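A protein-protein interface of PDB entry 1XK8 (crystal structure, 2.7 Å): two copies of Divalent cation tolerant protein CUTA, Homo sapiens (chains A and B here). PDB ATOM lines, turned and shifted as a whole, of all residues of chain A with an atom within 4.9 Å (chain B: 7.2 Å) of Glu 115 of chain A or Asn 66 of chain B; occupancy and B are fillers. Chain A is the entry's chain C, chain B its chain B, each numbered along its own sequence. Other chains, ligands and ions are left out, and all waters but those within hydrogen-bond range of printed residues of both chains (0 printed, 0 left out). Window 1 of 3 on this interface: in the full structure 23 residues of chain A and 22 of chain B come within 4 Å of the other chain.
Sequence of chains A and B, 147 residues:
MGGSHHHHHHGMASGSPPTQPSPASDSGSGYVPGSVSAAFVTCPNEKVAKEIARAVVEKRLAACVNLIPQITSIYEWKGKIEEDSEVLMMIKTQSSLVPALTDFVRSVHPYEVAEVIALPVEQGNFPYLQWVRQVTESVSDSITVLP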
ATOM      1  N   PHE A  40      20.635  -3.951  -3.827  1.00  0.00           N
ATOM      2  CA  PHE A  40      21.687  -3.930  -2.813  1.00  0.00           C
ATOM      3  C   PHE A  40      22.287  -5.303  -2.627  1.00  0.00           C
ATOM      4  O   PHE A  40      21.560  -6.273  -2.413  1.00  0.00           O
ATOM      5  CB  PHE A  40      21.143  -3.443  -1.472  1.00  0.00           C
ATOM      6  CG  PHE A  40      21.003  -1.952  -1.383  1.00  0.00           C
ATOM      7  CD1 PHE A  40      19.764  -1.335  -1.560  1.00  0.00           C
ATOM      8  CD2 PHE A  40      22.113  -1.157  -1.127  1.00  0.00           C
ATOM      9  CE1 PHE A  40      19.647   0.045  -1.475  1.00  0.00           C
ATOM     10  CE2 PHE A  40      21.997   0.223  -1.053  1.00  0.00           C
ATOM     11  CZ  PHE A  40      20.760   0.821  -1.222  1.00  0.00           C
ATOM     12  N   VAL A  41      23.615  -5.388  -2.702  1.00  0.00           N
ATOM     13  CA  VAL A  41      24.314  -6.651  -2.516  1.00  0.00           C
ATOM     14  C   VAL A  41      25.439  -6.492  -1.516  1.00  0.00           C
ATOM     15  O   VAL A  41      26.263  -5.597  -1.646  1.00  0.00           O
ATOM     16  CB  VAL A  41      24.926  -7.146  -3.831  1.00  0.00           C
ATOM     17  CG1 VAL A  41      25.649  -8.489  -3.622  1.00  0.00           C
ATOM     18  CG2 VAL A  41      23.846  -7.262  -4.910  1.00  0.00           C
ATOM     19  N   THR A  42      25.482  -7.383  -0.534  1.00  0.00           N
ATOM     20  CA  THR A  42      26.535  -7.377   0.474  1.00  0.00           C
ATOM     21  C   THR A  42      27.677  -8.327   0.100  1.00  0.00           C
ATOM     22  O   THR A  42      27.441  -9.469  -0.289  1.00  0.00           O
ATOM     23  CB  THR A  42      25.974  -7.787   1.832  1.00  0.00           C
ATOM     24  OG1 THR A  42      24.999  -6.822   2.235  1.00  0.00           O
ATOM     25  CG2 THR A  42      27.064  -7.861   2.883  1.00  0.00           C
ATOM     26  N   ILE A  71      31.640  -1.232   5.997  1.00  0.00           N
ATOM     27  CA  ILE A  71      30.341  -1.620   6.535  1.00  0.00           C
ATOM     28  C   ILE A  71      30.535  -2.616   7.680  1.00  0.00           C
ATOM     29  O   ILE A  71      31.390  -3.501   7.608  1.00  0.00           O
ATOM     30  CB  ILE A  71      29.449  -2.286   5.407  1.00  0.00           C
ATOM     31  CG1 ILE A  71      29.311  -1.361   4.191  1.00  0.00           C
ATOM     32  CG2 ILE A  71      28.066  -2.686   5.923  1.00  0.00           C
ATOM     33  CD1 ILE A  71      28.325  -0.241   4.371  1.00  0.00           C
ATOM     34  N   THR A  72      29.745  -2.466   8.737  1.00  0.00           N
ATOM     35  CA  THR A  72      29.679  -3.454   9.810  1.00  0.00           C
ATOM     36  C   THR A  72      28.331  -4.170   9.732  1.00  0.00           C
ATOM     37  O   THR A  72      27.284  -3.543   9.936  1.00  0.00           O
ATOM     38  CB  THR A  72      29.785  -2.802  11.222  1.00  0.00           C
ATOM     39  OG1 THR A  72      30.931  -1.963  11.296  1.00  0.00           O
ATOM     40  CG2 THR A  72      29.887  -3.859  12.303  1.00  0.00           C
ATOM     41  N   SER A  73      28.346  -5.471   9.443  1.00  0.00           N
ATOM     42  CA  SER A  73      27.109  -6.236   9.369  1.00  0.00           C
ATOM     43  C   SER A  73      26.849  -6.944  10.691  1.00  0.00           C
ATOM     44  O   SER A  73      27.764  -7.535  11.270  1.00  0.00           O
ATOM     45  CB  SER A  73      27.159  -7.224   8.205  1.00  0.00           C
ATOM     46  OG  SER A  73      27.091  -6.531   6.951  1.00  0.00           O
ATOM     47  N   LEU A  88      29.126  -2.884   0.675  1.00  0.00           N
ATOM     48  CA  LEU A  88      27.764  -2.874   0.155  1.00  0.00           C
ATOM     49  C   LEU A  88      27.747  -2.316  -1.262  1.00  0.00           C
ATOM     50  O   LEU A  88      28.340  -1.287  -1.539  1.00  0.00           O
ATOM     51  CB  LEU A  88      26.870  -2.032   1.081  1.00  0.00           C
ATOM     52  CG  LEU A  88      25.341  -2.068   0.896  1.00  0.00           C
ATOM     53  CD1 LEU A  88      24.763  -3.408   1.268  1.00  0.00           C
ATOM     54  CD2 LEU A  88      24.661  -0.975   1.716  1.00  0.00           C
ATOM     55  N   VAL A 113      24.204 -18.230   0.705  1.00  0.00           N
ATOM     56  CA  VAL A 113      22.988 -17.416   0.477  1.00  0.00           C
ATOM     57  C   VAL A 113      23.344 -15.913   0.365  1.00  0.00           C
ATOM     58  O   VAL A 113      23.598 -15.233   1.373  1.00  0.00           O
ATOM     59  CB  VAL A 113      21.945 -17.608   1.585  1.00  0.00           C
ATOM     60  N   ALA A 114      23.361 -15.414  -0.873  1.00  0.00           N
ATOM     61  CA  ALA A 114      23.743 -14.033  -1.167  1.00  0.00           C
ATOM     62  C   ALA A 114      22.596 -13.051  -0.901  1.00  0.00           C
ATOM     63  O   ALA A 114      21.468 -13.302  -1.325  1.00  0.00           O
ATOM     64  CB  ALA A 114      24.196 -13.931  -2.652  1.00  0.00           C
ATOM     65  N   GLU A 115      22.882 -11.941  -0.204  1.00  0.00           N
ATOM     66  CA  GLU A 115      21.903 -10.855  -0.083  1.00  0.00           C
ATOM     67  C   GLU A 115      21.778 -10.143  -1.420  1.00  0.00           C
ATOM     68  O   GLU A 115      22.736  -9.536  -1.895  1.00  0.00           O
ATOM     69  CB  GLU A 115      22.284  -9.810   0.989  1.00  0.00           C
ATOM     70  CG  GLU A 115      21.299  -8.567   1.010  1.00  0.00           C
ATOM     71  CD  GLU A 115      21.530  -7.585   2.179  1.00  0.00           C
ATOM     72  OE1 GLU A 115      22.658  -7.052   2.304  1.00  0.00           O
ATOM     73  OE2 GLU A 115      20.573  -7.320   2.956  1.00  0.00           O
ATOM     74  N   VAL A 116      20.605 -10.228  -2.032  1.00  0.00           N
ATOM     75  CA  VAL A 116      20.280  -9.378  -3.169  1.00  0.00           C
ATOM     76  C   VAL A 116      18.857  -8.890  -2.980  1.00  0.00           C
ATOM     77  O   VAL A 116      17.928  -9.680  -3.001  1.00  0.00           O
ATOM     78  CB  VAL A 116      20.432 -10.098  -4.511  1.00  0.00           C
ATOM     79  CG1 VAL A 116      20.182  -9.129  -5.669  1.00  0.00           C
ATOM     80  CG2 VAL A 116      21.811 -10.709  -4.622  1.00  0.00           C
ATOM     81  N   ILE A 117      18.704  -7.586  -2.766  1.00  0.00           N
ATOM     82  CA  ILE A 117      17.390  -6.977  -2.594  1.00  0.00           C
ATOM     83  C   ILE A 117      17.238  -5.788  -3.532  1.00  0.00           C
ATOM     84  O   ILE A 117      18.112  -4.956  -3.624  1.00  0.00           O
ATOM     85  CB  ILE A 117      17.139  -6.558  -1.133  1.00  0.00           C
ATOM     86  CG1 ILE A 117      18.260  -5.654  -0.610  1.00  0.00           C
ATOM     87  CG2 ILE A 117      17.016  -7.794  -0.261  1.00  0.00           C
ATOM     88  CD1 ILE A 117      17.960  -5.014   0.720  1.00  0.00           C
ATOM     89  N   ALA B  38      13.675  -2.690   3.791  1.00  0.00           N
ATOM     90  CA  ALA B  38      14.966  -2.187   4.245  1.00  0.00           C
ATOM     91  C   ALA B  38      14.705  -0.859   4.920  1.00  0.00           C
ATOM     92  O   ALA B  38      14.315   0.105   4.266  1.00  0.00           O
ATOM     93  CB  ALA B  38      15.897  -1.998   3.087  1.00  0.00           C
ATOM     94  N   ALA B  39      14.899  -0.815   6.231  1.00  0.00           N
ATOM     95  CA  ALA B  39      14.627   0.384   7.017  1.00  0.00           C
ATOM     96  C   ALA B  39      15.923   1.112   7.290  1.00  0.00           C
ATOM     97  O   ALA B  39      16.929   0.487   7.621  1.00  0.00           O
ATOM     98  CB  ALA B  39      13.929   0.029   8.323  1.00  0.00           C
ATOM     99  N   PHE B  40      15.901   2.432   7.151  1.00  0.00           N
ATOM    100  CA  PHE B  40      17.088   3.252   7.389  1.00  0.00           C
ATOM    101  C   PHE B  40      16.936   4.048   8.660  1.00  0.00           C
ATOM    102  O   PHE B  40      15.935   4.742   8.845  1.00  0.00           O
ATOM    103  CB  PHE B  40      17.340   4.201   6.230  1.00  0.00           C
ATOM    104  CG  PHE B  40      17.917   3.543   5.043  1.00  0.00           C
ATOM    105  CD1 PHE B  40      17.101   3.054   4.040  1.00  0.00           C
ATOM    106  CD2 PHE B  40      19.282   3.403   4.914  1.00  0.00           C
ATOM    107  CE1 PHE B  40      17.641   2.449   2.931  1.00  0.00           C
ATOM    108  CE2 PHE B  40      19.822   2.795   3.807  1.00  0.00           C
ATOM    109  CZ  PHE B  40      19.002   2.324   2.816  1.00  0.00           C
ATOM    110  N   VAL B  41      17.939   3.960   9.531  1.00  0.00           N
ATOM    111  CA  VAL B  41      17.926   4.694  10.797  1.00  0.00           C
ATOM    112  C   VAL B  41      19.236   5.437  11.004  1.00  0.00           C
ATOM    113  O   VAL B  41      20.312   4.849  10.896  1.00  0.00           O
ATOM    114  CB  VAL B  41      17.688   3.764  11.993  1.00  0.00           C
ATOM    115  CG1 VAL B  41      17.630   4.565  13.284  1.00  0.00           C
ATOM    116  CG2 VAL B  41      16.408   2.956  11.799  1.00  0.00           C
ATOM    117  N   ALA B  53      21.495  -1.843  16.956  1.00  0.00           N
ATOM    118  CA  ALA B  53      21.609  -2.935  15.996  1.00  0.00           C
ATOM    119  C   ALA B  53      21.571  -4.290  16.675  1.00  0.00           C
ATOM    120  O   ALA B  53      20.790  -5.167  16.287  1.00  0.00           O
ATOM    121  CB  ALA B  53      22.898  -2.804  15.212  1.00  0.00           C
ATOM    122  N   CYS B  64      18.986  -8.714  10.003  1.00  0.00           N
ATOM    123  CA  CYS B  64      20.333  -8.175  10.148  1.00  0.00           C
ATOM    124  C   CYS B  64      20.382  -6.689   9.849  1.00  0.00           C
ATOM    125  O   CYS B  64      19.436  -6.113   9.297  1.00  0.00           O
ATOM    126  CB  CYS B  64      21.286  -8.872   9.214  1.00  0.00           C
ATOM    127  SG  CYS B  64      20.848  -8.587   7.549  1.00  0.00           S
ATOM    128  N   VAL B  65      21.513  -6.091  10.191  1.00  0.00           N
ATOM    129  CA  VAL B  65      21.692  -4.668  10.101  1.00  0.00           C
ATOM    130  C   VAL B  65      23.042  -4.379   9.479  1.00  0.00           C
ATOM    131  O   VAL B  65      24.043  -4.958   9.891  1.00  0.00           O
ATOM    132  CB  VAL B  65      21.632  -4.051  11.526  1.00  0.00           C
ATOM    133  CG1 VAL B  65      21.858  -2.554  11.498  1.00  0.00           C
ATOM    134  CG2 VAL B  65      20.291  -4.390  12.199  1.00  0.00           C
ATOM    135  N   ASN B  66      23.065  -3.489   8.489  1.00  0.00           N
ATOM    136  CA  ASN B  66      24.314  -2.959   7.939  1.00  0.00           C
ATOM    137  C   ASN B  66      24.559  -1.562   8.484  1.00  0.00           C
ATOM    138  O   ASN B  66      23.665  -0.722   8.461  1.00  0.00           O
ATOM    139  CB  ASN B  66      24.230  -2.893   6.420  1.00  0.00           C
ATOM    140  CG  ASN B  66      23.986  -4.235   5.800  1.00  0.00           C
ATOM    141  OD1 ASN B  66      24.666  -5.192   6.115  1.00  0.00           O
ATOM    142  ND2 ASN B  66      23.019  -4.313   4.911  1.00  0.00           N
ATOM    143  N   LEU B  67      25.767  -1.318   8.977  1.00  0.00           N
ATOM    144  CA  LEU B  67      26.140  -0.005   9.497  1.00  0.00           C
ATOM    145  C   LEU B  67      27.035   0.708   8.512  1.00  0.00           C
ATOM    146  O   LEU B  67      28.079   0.195   8.137  1.00  0.00           O
ATOM    147  CB  LEU B  67      26.860  -0.144  10.828  1.00  0.00           C
ATOM    148  CG  LEU B  67      25.953  -0.162  12.051  1.00  0.00           C
ATOM    149  CD1 LEU B  67      24.976  -1.280  11.959  1.00  0.00           C
ATOM    150  CD2 LEU B  67      26.793  -0.271  13.321  1.00  0.00           C
ATOM    151  N   ILE B  68      26.617   1.900   8.096  1.00  0.00           N
ATOM    152  CA  ILE B  68      27.395   2.718   7.180  1.00  0.00           C
ATOM    153  C   ILE B  68      27.930   3.919   7.963  1.00  0.00           C
ATOM    154  O   ILE B  68      27.151   4.788   8.370  1.00  0.00           O
ATOM    155  CB  ILE B  68      26.534   3.172   5.989  1.00  0.00           C
ATOM    156  CG1 ILE B  68      25.701   1.992   5.450  1.00  0.00           C
ATOM    157  CG2 ILE B  68      27.416   3.744   4.893  1.00  0.00           C
ATOM    158  CD1 ILE B  68      24.451   2.389   4.697  1.00  0.00           C
ATOM    159  N   VAL B  87      26.029   7.957  11.874  1.00  0.00           N
ATOM    160  CA  VAL B  87      26.148   6.600  11.333  1.00  0.00           C
ATOM    161  C   VAL B  87      24.776   6.154  10.870  1.00  0.00           C
ATOM    162  O   VAL B  87      23.781   6.428  11.532  1.00  0.00           O
ATOM    163  CB  VAL B  87      26.708   5.610  12.367  1.00  0.00           C
ATOM    164  CG1 VAL B  87      26.585   4.148  11.858  1.00  0.00           C
ATOM    165  CG2 VAL B  87      28.168   5.961  12.690  1.00  0.00           C
ATOM    166  N   LEU B  88      24.732   5.467   9.735  1.00  0.00           N
ATOM    167  CA  LEU B  88      23.476   5.081   9.109  1.00  0.00           C
ATOM    168  C   LEU B  88      23.281   3.558   9.174  1.00  0.00           C
ATOM    169  O   LEU B  88      24.180   2.787   8.823  1.00  0.00           O
ATOM    170  CB  LEU B  88      23.475   5.577   7.660  1.00  0.00           C
ATOM    171  CG  LEU B  88      22.205   5.454   6.831  1.00  0.00           C
ATOM    172  CD1 LEU B  88      20.989   6.012   7.570  1.00  0.00           C
ATOM    173  CD2 LEU B  88      22.414   6.159   5.510  1.00  0.00           C
ATOM    174  N   MET B  89      22.105   3.137   9.636  1.00  0.00           N
ATOM    175  CA  MET B  89      21.762   1.731   9.709  1.00  0.00           C
ATOM    176  C   MET B  89      20.852   1.376   8.563  1.00  0.00           C
ATOM    177  O   MET B  89      19.865   2.058   8.328  1.00  0.00           O
ATOM    178  CB  MET B  89      21.019   1.427  11.001  1.00  0.00           C
ATOM    179  CG  MET B  89      21.762   1.745  12.258  1.00  0.00           C
ATOM    180  SD  MET B  89      20.688   1.522  13.696  1.00  0.00           S
ATOM    181  CE  MET B  89      20.777  -0.244  13.918  1.00  0.00           C
ATOM    182  N   MET B  90      21.178   0.304   7.850  1.00  0.00           N
ATOM    183  CA  MET B  90      20.223  -0.307   6.931  1.00  0.00           C
ATOM    184  C   MET B  90      19.762  -1.621   7.535  1.00  0.00           C
ATOM    185  O   MET B  90      20.509  -2.589   7.590  1.00  0.00           O
ATOM    186  CB  MET B  90      20.801  -0.516   5.548  1.00  0.00           C
ATOM    187  CG  MET B  90      19.731  -0.816   4.547  1.00  0.00           C
ATOM    188  SD  MET B  90      20.312  -0.866   2.882  1.00  0.00           S
ATOM    189  CE  MET B  90      21.129  -2.465   2.857  1.00  0.00           C
ATOM    190  N   ILE B  91      18.526  -1.626   8.006  1.00  0.00           N
ATOM    191  CA  ILE B  91      17.961  -2.753   8.751  1.00  0.00           C
ATOM    192  C   ILE B  91      17.048  -3.539   7.834  1.00  0.00           C
ATOM    193  O   ILE B  91      16.113  -2.976   7.276  1.00  0.00           O
ATOM    194  CB  ILE B  91      17.127  -2.256   9.960  1.00  0.00           C
ATOM    195  CG1 ILE B  91      17.954  -1.295  10.820  1.00  0.00           C
ATOM    196  CG2 ILE B  91      16.633  -3.437  10.786  1.00  0.00           C
ATOM    197  CD1 ILE B  91      17.133  -0.436  11.758  1.00  0.00           C
ATOM    198  N   LYS B  92      17.316  -4.835   7.673  1.00  0.00           N
ATOM    199  CA  LYS B  92      16.512  -5.684   6.777  1.00  0.00           C
ATOM    200  C   LYS B  92      15.588  -6.562   7.609  1.00  0.00           C
ATOM    201  O   LYS B  92      16.042  -7.326   8.448  1.00  0.00           O
ATOM    202  CB  LYS B  92      17.400  -6.526   5.853  1.00  0.00           C
ATOM    203  N   GLY B 124      14.165  -9.913  -5.309  1.00  0.00           N
ATOM    204  CA  GLY B 124      15.454 -10.289  -4.711  1.00  0.00           C
ATOM    205  C   GLY B 124      15.797 -11.763  -4.762  1.00  0.00           C
ATOM    206  O   GLY B 124      15.176 -12.527  -5.483  1.00  0.00           O
ATOM    207  N   ASN B 125      16.813 -12.151  -3.995  1.00  0.00           N
ATOM    208  CA  ASN B 125      17.213 -13.552  -3.863  1.00  0.00           C
ATOM    209  C   ASN B 125      16.249 -14.276  -2.930  1.00  0.00           C
ATOM    210  O   ASN B 125      16.282 -14.071  -1.712  1.00  0.00           O
ATOM    211  CB  ASN B 125      18.649 -13.640  -3.323  1.00  0.00           C
ATOM    212  CG  ASN B 125      19.342 -14.940  -3.698  1.00  0.00           C
ATOM    213  OD1 ASN B 125      18.749 -15.817  -4.314  1.00  0.00           O
ATOM    214  ND2 ASN B 125      20.618 -15.059  -3.334  1.00  0.00           N
ATOM    215  N   TYR B 128      17.317 -15.799   0.436  1.00  0.00           N
ATOM    216  CA  TYR B 128      17.659 -14.758   1.395  1.00  0.00           C
ATOM    217  C   TYR B 128      16.413 -14.077   1.937  1.00  0.00           C
ATOM    218  O   TYR B 128      16.298 -13.837   3.134  1.00  0.00           O
ATOM    219  CB  TYR B 128      18.577 -13.717   0.754  1.00  0.00           C
ATOM    220  CG  TYR B 128      18.998 -12.616   1.700  1.00  0.00           C
ATOM    221  CD1 TYR B 128      18.319 -11.389   1.725  1.00  0.00           C
ATOM    222  CD2 TYR B 128      20.068 -12.799   2.586  1.00  0.00           C
ATOM    223  CE1 TYR B 128      18.694 -10.385   2.589  1.00  0.00           C
ATOM    224  CE2 TYR B 128      20.456 -11.785   3.460  1.00  0.00           C
ATOM    225  CZ  TYR B 128      19.764 -10.580   3.454  1.00  0.00           C
ATOM    226  OH  TYR B 128      20.148  -9.566   4.317  1.00  0.00           O
ATOM    227  N   LEU B 129      15.476 -13.772   1.046  1.00  0.00           N
ATOM    228  CA  LEU B 129      14.189 -13.175   1.450  1.00  0.00           C
ATOM    229  C   LEU B 129      13.399 -14.123   2.363  1.00  0.00           C
ATOM    230  O   LEU B 129      12.774 -13.692   3.330  1.00  0.00           O
ATOM    231  CB  LEU B 129      13.381 -12.794   0.213  1.00  0.00           C
ATOM    232  CG  LEU B 129      14.062 -11.788  -0.740  1.00  0.00           C
ATOM    233  CD1 LEU B 129      13.285 -11.650  -2.038  1.00  0.00           C
ATOM    234  CD2 LEU B 129      14.239 -10.429  -0.078  1.00  0.00           C
ATOM    235  N   TRP B 131      14.907 -16.369   4.264  1.00  0.00           N
ATOM    236  CA  TRP B 131      15.711 -16.348   5.482  1.00  0.00           C
ATOM    237  C   TRP B 131      15.357 -15.178   6.410  1.00  0.00           C
ATOM    238  O   TRP B 131      15.284 -15.349   7.625  1.00  0.00           O
ATOM    239  CB  TRP B 131      17.206 -16.292   5.131  1.00  0.00           C
ATOM    240  CG  TRP B 131      18.054 -16.101   6.316  1.00  0.00           C
ATOM    241  CD1 TRP B 131      18.299 -17.016   7.300  1.00  0.00           C
ATOM    242  CD2 TRP B 131      18.768 -14.912   6.688  1.00  0.00           C
ATOM    243  NE1 TRP B 131      19.123 -16.473   8.256  1.00  0.00           N
ATOM    244  CE2 TRP B 131      19.426 -15.184   7.905  1.00  0.00           C
ATOM    245  CE3 TRP B 131      18.919 -13.647   6.107  1.00  0.00           C
ATOM    246  CZ2 TRP B 131      20.226 -14.244   8.552  1.00  0.00           C
ATOM    247  CZ3 TRP B 131      19.721 -12.703   6.760  1.00  0.00           C
ATOM    248  CH2 TRP B 131      20.361 -13.013   7.966  1.00  0.00           C
ATOM    249  N   VAL B 132      15.155 -13.990   5.832  1.00  0.00           N
ATOM    250  CA  VAL B 132      14.768 -12.801   6.610  1.00  0.00           C
ATOM    251  C   VAL B 132      13.463 -13.052   7.355  1.00  0.00           C
ATOM    252  O   VAL B 132      13.309 -12.627   8.496  1.00  0.00           O
ATOM    253  CB  VAL B 132      14.612 -11.527   5.700  1.00  0.00           C
ATOM    254  CG1 VAL B 132      13.951 -10.367   6.466  1.00  0.00           C
ATOM    255  CG2 VAL B 132      15.954 -11.083   5.150  1.00  0.00           C
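The side-chain amide oxygen (OD1) of Asn 66 of chain B lies within hydrogen-bond range of the side-chain hydroxyl (OG) of Ser 73 of chain A (2.9 Å). The backbone NH (N) of Leu 67 of chain B lies within hydrogen-bond range of the backbone carbonyl oxygen (O) of Thr 72 of chain A. ND2 of Asn 125 of chain B lies within hydrogen-bond range of O of Ala 114 of chain A (2.8 Å). The backbone NH (N) of Asn 125 of chain B lies within hydrogen-bond range of the backbone carbonyl oxygen (O) of Val 116 of chain A, 2.9 Å away. The side-chain carboxylate of Glu 115 of chain A sits at hydrogen-bond distance from the side-chain hydroxyl of Tyr 128 of chain B, 2.7 Å away.
The side-chain sulfur of Cys 64 of chain B is in hydrogen-bond range of the side-chain hydroxyl of Tyr 128 of chain B. The backbone NH (N) of Met 90 of chain B sits at hydrogen-bond distance from the backbone carbonyl oxygen (O) of Asn 66 of chain B (2.8 Å). The backbone carbonyl oxygen (O) of Leu 88 of chain B sits at hydrogen-bond distance from the backbone NH (N) of Ile 68 of chain B (2.7 Å). O of Ile 117 of chain A is in hydrogen-bond range of N of Phe 40 of chain A (2.7 Å).
Among the printed residues, merely in contact across the chains: Val 116 of chain A with Gly 124 of chain B (3.1 Å), Ile 71 of chain A with Leu 67 of chain B (3.3 Å), Ser 73 of chain A with Val 65 of chain B (3.4 Å), Thr 72 of chain A with Val 65 of chain B (3.5 Å), Ala 114 of chain A with Tyr 128 of chain B (3.6 Å), Ile 71 of chain A with Ile 68 of chain B (3.6 Å), Thr 72 of chain A with Asn 66 of chain B (3.6 Å), Glu 115 of chain A with Asn 66 of chain B (3.8 Å), Ile 117 of chain A with Leu 129 of chain B (3.8 Å), Ile 71 of chain A with Asn 66 of chain B (3.9 Å) and Leu 88 of chain A with Met 90 of chain B (3.9996 Å).
Of chain B, only Asn 66 and Tyr 128 come within 4 Å of Glu 115 of chain A. Asn 66 of chain B touches just these residues of chain A: Ile 71, Thr 72, Ser 73 and Glu 115. Printed residues of chain A within 4 Å of Ile 68 of chain B: Ile 71. Of the printed residues of chain A, Met 90 of chain B touches Leu 88. Trp 131 of chain B touches none of the printed residues of chain A. Ala 39 of chain B touches none of the printed residues of chain A. The nearest printed residue of chain A that does not touch Asn 66 of chain B is Leu 88 of chain A (4.1 Å).
Hydrophobic or aromatic side chains of chain B that line the printed part of chain A: Leu 67, Ile 68, Met 90, Tyr 128 and Leu 129. Printed residues of chain A that touch a printed residue of chain B: Ile 71, Thr 72, Ser 73, Leu 88, Ala 114, Glu 115, Val 116 and Ile 117. Among the printed residues, 16 pairs touch across the chains.
Positions printed for both chains: 40, 41 and 88.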
